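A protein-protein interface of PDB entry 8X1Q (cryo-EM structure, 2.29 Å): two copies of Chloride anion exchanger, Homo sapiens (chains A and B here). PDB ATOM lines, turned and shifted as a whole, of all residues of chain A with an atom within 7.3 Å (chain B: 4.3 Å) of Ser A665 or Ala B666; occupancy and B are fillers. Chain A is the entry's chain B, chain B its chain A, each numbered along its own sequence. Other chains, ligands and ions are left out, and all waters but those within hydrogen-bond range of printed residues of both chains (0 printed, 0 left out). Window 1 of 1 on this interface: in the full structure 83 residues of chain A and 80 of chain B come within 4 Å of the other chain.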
ATOM      1  N   ARG A 550      -5.522  -4.271  12.786  1.00  0.00           N
ATOM      2  CA  ARG A 550      -6.722  -3.588  12.310  1.00  0.00           C
ATOM      3  C   ARG A 550      -6.344  -2.330  11.538  1.00  0.00           C
ATOM      4  O   ARG A 550      -5.457  -1.584  11.959  1.00  0.00           O
ATOM      5  CB  ARG A 550      -7.645  -3.246  13.481  1.00  0.00           C
ATOM      6  CG  ARG A 550      -8.709  -2.225  13.170  1.00  0.00           C
ATOM      7  CD  ARG A 550      -9.610  -1.988  14.359  1.00  0.00           C
ATOM      8  NE  ARG A 550     -10.480  -0.836  14.160  1.00  0.00           N
ATOM      9  CZ  ARG A 550     -11.725  -0.901  13.704  1.00  0.00           C
ATOM     10  NH1 ARG A 550     -12.435   0.203  13.555  1.00  0.00           N
ATOM     11  NH2 ARG A 550     -12.265  -2.070  13.396  1.00  0.00           N
ATOM     12  N   CYS A 551      -7.018  -2.100  10.406  1.00  0.00           N
ATOM     13  CA  CYS A 551      -6.884  -0.888   9.604  1.00  0.00           C
ATOM     14  C   CYS A 551      -8.259  -0.267   9.400  1.00  0.00           C
ATOM     15  O   CYS A 551      -9.128  -0.896   8.782  1.00  0.00           O
ATOM     16  CB  CYS A 551      -6.238  -1.196   8.256  1.00  0.00           C
ATOM     17  SG  CYS A 551      -6.066   0.222   7.153  1.00  0.00           S
ATOM     18  N   PRO A 552      -8.509   0.931   9.907  1.00  0.00           N
ATOM     19  CA  PRO A 552      -9.872   1.500   9.925  1.00  0.00           C
ATOM     20  C   PRO A 552     -10.211   2.377   8.718  1.00  0.00           C
ATOM     21  O   PRO A 552     -10.665   3.516   8.873  1.00  0.00           O
ATOM     22  CB  PRO A 552      -9.870   2.301  11.215  1.00  0.00           C
ATOM     23  CG  PRO A 552      -8.456   2.791  11.328  1.00  0.00           C
ATOM     24  CD  PRO A 552      -7.562   1.816  10.597  1.00  0.00           C
ATOM     25  N   SER A 553      -9.988   1.865   7.520  1.00  0.00           N
ATOM     26  CA  SER A 553     -10.216   2.635   6.312  1.00  0.00           C
ATOM     27  C   SER A 553     -10.222   1.733   5.104  1.00  0.00           C
ATOM     28  O   SER A 553      -9.802   0.602   5.187  1.00  0.00           O
ATOM     29  CB  SER A 553      -9.016   3.585   6.132  1.00  0.00           C
ATOM     30  OG  SER A 553      -9.230   4.598   5.174  1.00  0.00           O
ATOM     31  N   PRO A 554     -10.753   2.219   3.983  1.00  0.00           N
ATOM     32  CA  PRO A 554     -10.589   1.492   2.719  1.00  0.00           C
ATOM     33  C   PRO A 554      -9.142   1.514   2.248  1.00  0.00           C
ATOM     34  O   PRO A 554      -8.374   2.420   2.567  1.00  0.00           O
ATOM     35  CB  PRO A 554     -11.495   2.254   1.746  1.00  0.00           C
ATOM     36  CG  PRO A 554     -12.396   3.042   2.585  1.00  0.00           C
ATOM     37  CD  PRO A 554     -11.667   3.363   3.836  1.00  0.00           C
ATOM     38  N   LEU A 662      -6.471 -10.618  10.491  1.00  0.00           N
ATOM     39  CA  LEU A 662      -6.689  -9.263   9.981  1.00  0.00           C
ATOM     40  C   LEU A 662      -8.152  -8.855  10.080  1.00  0.00           C
ATOM     41  O   LEU A 662      -9.005  -9.483   9.472  1.00  0.00           O
ATOM     42  CB  LEU A 662      -6.230  -9.160   8.532  1.00  0.00           C
ATOM     43  CG  LEU A 662      -4.756  -9.438   8.237  1.00  0.00           C
ATOM     44  CD1 LEU A 662      -4.501  -9.348   6.742  1.00  0.00           C
ATOM     45  CD2 LEU A 662      -3.866  -8.471   8.996  1.00  0.00           C
ATOM     46  N   ASP A 663      -8.446  -7.812  10.848  1.00  0.00           N
ATOM     47  CA  ASP A 663      -9.818  -7.330  11.015  1.00  0.00           C
ATOM     48  C   ASP A 663     -10.196  -6.349   9.921  1.00  0.00           C
ATOM     49  O   ASP A 663      -9.648  -5.253   9.863  1.00  0.00           O
ATOM     50  CB  ASP A 663      -9.968  -6.678  12.393  1.00  0.00           C
ATOM     51  CG  ASP A 663     -11.352  -6.110  12.629  1.00  0.00           C
ATOM     52  OD1 ASP A 663     -12.310  -6.545  11.960  1.00  0.00           O
ATOM     53  OD2 ASP A 663     -11.482  -5.226  13.499  1.00  0.00           O
ATOM     54  N   PHE A 664     -11.145  -6.718   9.067  1.00  0.00           N
ATOM     55  CA  PHE A 664     -11.497  -5.874   7.923  1.00  0.00           C
ATOM     56  C   PHE A 664     -12.922  -5.326   7.957  1.00  0.00           C
ATOM     57  O   PHE A 664     -13.538  -5.151   6.921  1.00  0.00           O
ATOM     58  CB  PHE A 664     -11.291  -6.666   6.628  1.00  0.00           C
ATOM     59  CG  PHE A 664      -9.894  -6.601   6.082  1.00  0.00           C
ATOM     60  CD1 PHE A 664      -8.818  -6.347   6.909  1.00  0.00           C
ATOM     61  CD2 PHE A 664      -9.661  -6.805   4.734  1.00  0.00           C
ATOM     62  CE1 PHE A 664      -7.534  -6.291   6.401  1.00  0.00           C
ATOM     63  CE2 PHE A 664      -8.383  -6.752   4.218  1.00  0.00           C
ATOM     64  CZ  PHE A 664      -7.317  -6.494   5.054  1.00  0.00           C
ATOM     65  N   SER A 665     -13.439  -5.051   9.147  1.00  0.00           N
ATOM     66  CA  SER A 665     -14.794  -4.513   9.290  1.00  0.00           C
ATOM     67  C   SER A 665     -14.968  -3.086   8.748  1.00  0.00           C
ATOM     68  O   SER A 665     -16.018  -2.768   8.205  1.00  0.00           O
ATOM     69  CB  SER A 665     -15.227  -4.577  10.752  1.00  0.00           C
ATOM     70  OG  SER A 665     -14.319  -3.883  11.589  1.00  0.00           O
ATOM     71  N   ALA A 666     -13.955  -2.235   8.887  1.00  0.00           N
ATOM     72  CA  ALA A 666     -14.035  -0.858   8.397  1.00  0.00           C
ATOM     73  C   ALA A 666     -13.417  -0.655   7.015  1.00  0.00           C
ATOM     74  O   ALA A 666     -13.299   0.475   6.559  1.00  0.00           O
ATOM     75  CB  ALA A 666     -13.412   0.092   9.405  1.00  0.00           C
ATOM     76  N   VAL A 667     -13.022  -1.732   6.347  1.00  0.00           N
ATOM     77  CA  VAL A 667     -12.518  -1.628   4.981  1.00  0.00           C
ATOM     78  C   VAL A 667     -13.721  -1.699   4.065  1.00  0.00           C
ATOM     79  O   VAL A 667     -14.332  -2.753   3.942  1.00  0.00           O
ATOM     80  CB  VAL A 667     -11.515  -2.746   4.653  1.00  0.00           C
ATOM     81  CG1 VAL A 667     -10.992  -2.591   3.232  1.00  0.00           C
ATOM     82  CG2 VAL A 667     -10.368  -2.747   5.651  1.00  0.00           C
ATOM     83  N   SER A 668     -14.074  -0.595   3.418  1.00  0.00           N
ATOM     84  CA  SER A 668     -15.305  -0.563   2.616  1.00  0.00           C
ATOM     85  C   SER A 668     -15.162  -1.040   1.172  1.00  0.00           C
ATOM     86  O   SER A 668     -16.070  -1.676   0.651  1.00  0.00           O
ATOM     87  CB  SER A 668     -15.899   0.852   2.644  1.00  0.00           C
ATOM     88  OG  SER A 668     -15.984   1.343   3.969  1.00  0.00           O
ATOM     89  N   VAL A 695     -11.434 -11.632   8.952  1.00  0.00           N
ATOM     90  CA  VAL A 695     -12.709 -11.664   9.654  1.00  0.00           C
ATOM     91  C   VAL A 695     -13.411 -10.320   9.508  1.00  0.00           C
ATOM     92  O   VAL A 695     -12.793  -9.296   9.214  1.00  0.00           O
ATOM     93  CB  VAL A 695     -12.545 -12.022  11.147  1.00  0.00           C
ATOM     94  CG1 VAL A 695     -11.765 -13.305  11.308  1.00  0.00           C
ATOM     95  CG2 VAL A 695     -11.868 -10.898  11.898  1.00  0.00           C
ATOM     96  N   GLY A 696     -14.732 -10.316   9.704  1.00  0.00           N
ATOM     97  CA  GLY A 696     -15.487  -9.070   9.673  1.00  0.00           C
ATOM     98  C   GLY A 696     -16.060  -8.533   8.383  1.00  0.00           C
ATOM     99  O   GLY A 696     -16.413  -7.362   8.313  1.00  0.00           O
ATOM    100  N   THR A 697     -16.176  -9.368   7.364  1.00  0.00           N
ATOM    101  CA  THR A 697     -16.642  -8.893   6.065  1.00  0.00           C
ATOM    102  C   THR A 697     -18.059  -9.350   5.744  1.00  0.00           C
ATOM    103  O   THR A 697     -18.560 -10.289   6.352  1.00  0.00           O
ATOM    104  CB  THR A 697     -15.686  -9.346   4.946  1.00  0.00           C
ATOM    105  OG1 THR A 697     -15.636 -10.776   4.911  1.00  0.00           O
ATOM    106  CG2 THR A 697     -14.287  -8.804   5.187  1.00  0.00           C
ATOM    107  N   ASP A 698     -18.716  -8.681   4.803  1.00  0.00           N
ATOM    108  CA  ASP A 698     -20.066  -9.078   4.391  1.00  0.00           C
ATOM    109  C   ASP A 698     -20.051  -9.950   3.139  1.00  0.00           C
ATOM    110  O   ASP A 698     -18.992 -10.197   2.565  1.00  0.00           O
ATOM    111  CB  ASP A 698     -20.951  -7.849   4.176  1.00  0.00           C
ATOM    112  CG  ASP A 698     -20.438  -6.942   3.078  1.00  0.00           C
ATOM    113  OD1 ASP A 698     -19.286  -7.125   2.637  1.00  0.00           O
ATOM    114  OD2 ASP A 698     -21.187  -6.034   2.660  1.00  0.00           O
ATOM    115  N   PRO B 552     -23.044   0.589   4.387  1.00  0.00           N
ATOM    116  CA  PRO B 552     -21.668   0.109   4.263  1.00  0.00           C
ATOM    117  C   PRO B 552     -20.633   1.078   3.684  1.00  0.00           C
ATOM    118  O   PRO B 552     -19.877   0.635   2.841  1.00  0.00           O
ATOM    119  CB  PRO B 552     -21.839  -1.067   3.308  1.00  0.00           C
ATOM    120  CG  PRO B 552     -22.931  -0.624   2.396  1.00  0.00           C
ATOM    121  CD  PRO B 552     -23.813   0.327   3.160  1.00  0.00           C
ATOM    122  N   SER B 553     -20.551   2.313   4.166  1.00  0.00           N
ATOM    123  CA  SER B 553     -19.618   3.293   3.626  1.00  0.00           C
ATOM    124  C   SER B 553     -19.518   4.516   4.523  1.00  0.00           C
ATOM    125  O   SER B 553     -20.351   4.698   5.393  1.00  0.00           O
ATOM    126  CB  SER B 553     -20.192   3.782   2.290  1.00  0.00           C
ATOM    127  OG  SER B 553     -19.257   4.476   1.500  1.00  0.00           O
ATOM    128  N   PRO B 554     -18.481   5.356   4.329  1.00  0.00           N
ATOM    129  CA  PRO B 554     -18.444   6.646   5.034  1.00  0.00           C
ATOM    130  C   PRO B 554     -19.541   7.580   4.546  1.00  0.00           C
ATOM    131  O   PRO B 554     -20.011   7.482   3.412  1.00  0.00           O
ATOM    132  CB  PRO B 554     -17.057   7.202   4.691  1.00  0.00           C
ATOM    133  CG  PRO B 554     -16.284   6.057   4.209  1.00  0.00           C
ATOM    134  CD  PRO B 554     -17.238   5.112   3.582  1.00  0.00           C
ATOM    135  N   PHE B 664     -22.928   1.002  12.507  1.00  0.00           N
ATOM    136  CA  PHE B 664     -21.926   1.896  11.926  1.00  0.00           C
ATOM    137  C   PHE B 664     -20.543   1.277  11.877  1.00  0.00           C
ATOM    138  O   PHE B 664     -19.549   1.982  11.971  1.00  0.00           O
ATOM    139  CB  PHE B 664     -21.881   3.206  12.717  1.00  0.00           C
ATOM    140  CG  PHE B 664     -22.854   4.246  12.239  1.00  0.00           C
ATOM    141  CD1 PHE B 664     -24.047   3.881  11.644  1.00  0.00           C
ATOM    142  CD2 PHE B 664     -22.573   5.592  12.391  1.00  0.00           C
ATOM    143  CE1 PHE B 664     -24.939   4.839  11.203  1.00  0.00           C
ATOM    144  CE2 PHE B 664     -23.460   6.556  11.956  1.00  0.00           C
ATOM    145  CZ  PHE B 664     -24.648   6.179  11.360  1.00  0.00           C
ATOM    146  N   SER B 665     -20.475  -0.038  11.730  1.00  0.00           N
ATOM    147  CA  SER B 665     -19.196  -0.742  11.674  1.00  0.00           C
ATOM    148  C   SER B 665     -18.338  -0.395  10.450  1.00  0.00           C
ATOM    149  O   SER B 665     -17.117  -0.484  10.517  1.00  0.00           O
ATOM    150  CB  SER B 665     -19.459  -2.242  11.709  1.00  0.00           C
ATOM    151  OG  SER B 665     -18.251  -2.970  11.613  1.00  0.00           O
ATOM    152  N   ALA B 666     -18.963  -0.004   9.344  1.00  0.00           N
ATOM    153  CA  ALA B 666     -18.233   0.334   8.122  1.00  0.00           C
ATOM    154  C   ALA B 666     -18.178   1.834   7.817  1.00  0.00           C
ATOM    155  O   ALA B 666     -17.672   2.220   6.772  1.00  0.00           O
ATOM    156  CB  ALA B 666     -18.820  -0.430   6.945  1.00  0.00           C
ATOM    157  N   VAL B 667     -18.697   2.673   8.708  1.00  0.00           N
ATOM    158  CA  VAL B 667     -18.590   4.123   8.534  1.00  0.00           C
ATOM    159  C   VAL B 667     -17.224   4.531   9.051  1.00  0.00           C
ATOM    160  O   VAL B 667     -16.975   4.452  10.249  1.00  0.00           O
ATOM    161  CB  VAL B 667     -19.724   4.877   9.251  1.00  0.00           C
ATOM    162  CG1 VAL B 667     -19.597   6.374   9.024  1.00  0.00           C
ATOM    163  CG2 VAL B 667     -21.077   4.374   8.775  1.00  0.00           C
ATOM    164  N   SER B 668     -16.341   4.989   8.176  1.00  0.00           N
ATOM    165  CA  SER B 668     -14.962   5.269   8.563  1.00  0.00           C
ATOM    166  C   SER B 668     -14.793   6.693   9.082  1.00  0.00           C
ATOM    167  O   SER B 668     -14.071   6.919  10.061  1.00  0.00           O
ATOM    168  CB  SER B 668     -14.018   5.007   7.392  1.00  0.00           C
ATOM    169  OG  SER B 668     -14.380   3.827   6.707  1.00  0.00           O
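OG of Ser A668 is in hydrogen-bond range of O of Ala B666, at 3.4 Å. The backbone carbonyl oxygen of Ser B665 lies close to the backbone carbonyl oxygen of Ser A665, at 3.4 Å.
NH2 of Arg A550 is in hydrogen-bond range of OG of Ser A665, at 3.3 Å. OD1 of Asp A663 sits at hydrogen-bond distance from OG of Ser A665 (3.4 Å).
CB of Ser B668 touches O of Pro A552, at 3.96 Å. OG of Ser B668 touches CD of Pro A554, 3.98 Å away. Ser A665 touches Ala B666 (O to CA, 3.8 Å). CA of Ala A666 touches O of Ser B665 (3.8 Å). O of Ala A666 touches OG of Ser B668 (3.5 Å). Ser A668 touches Pro B552. Ser A668 touches Pro B554 (OG to CD, 3.99 Å).
Of chain B, only Ser B665 (3.4 Å) and Ala B666 (3.8 Å) come within 4 Å of Ser A665. Ala B666 touches two residues of chain A. Of the printed residues of chain A, Pro B552 touches Ser A668 (3.99 Å). Printed residues of chain B within 4 Å of Ala A666: Ser B665 and Ser B668. Of the printed residues of chain B, Pro A554 touches Ser B668 (3.98 Å). Of the printed residues of chain A, Pro B554 touches Ser A668. The nearest printed residue of chain B that does not touch Pro A554 is Pro B554 (5.2 Å).
Of the 16 printed residues of chain A, 5 touch a printed residue of chain B. Printed residues of chain A that touch a printed residue of chain B: Pro A552, Pro A554, Ser A665, Ala A666 and Ser A668. Hydrophobic or aromatic side chains of chain A that line the printed part of chain B: Pro A554 and Ala A666. Along chain A the printed residues that touch a printed residue of chain B span positions 552 to 668.
Pro A552 touches Ser B668, and with the chains exchanged Ser A668 touches Pro B552. Pro A554 touches Ser B668, and with the chains exchanged Ser A668 touches Pro B554. Ser A665 touches its own counterpart, Ser B665. Ser A665 touches Ala B666, and with the chains exchanged Ala A666 touches Ser B665. Positions printed for both chains: 552, 553, 554, 664, 665, 666, 667 and 668. Of the 9 pairs that touch across the chains among the printed residues, 9 have their exchanged pair printed and touching as well.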
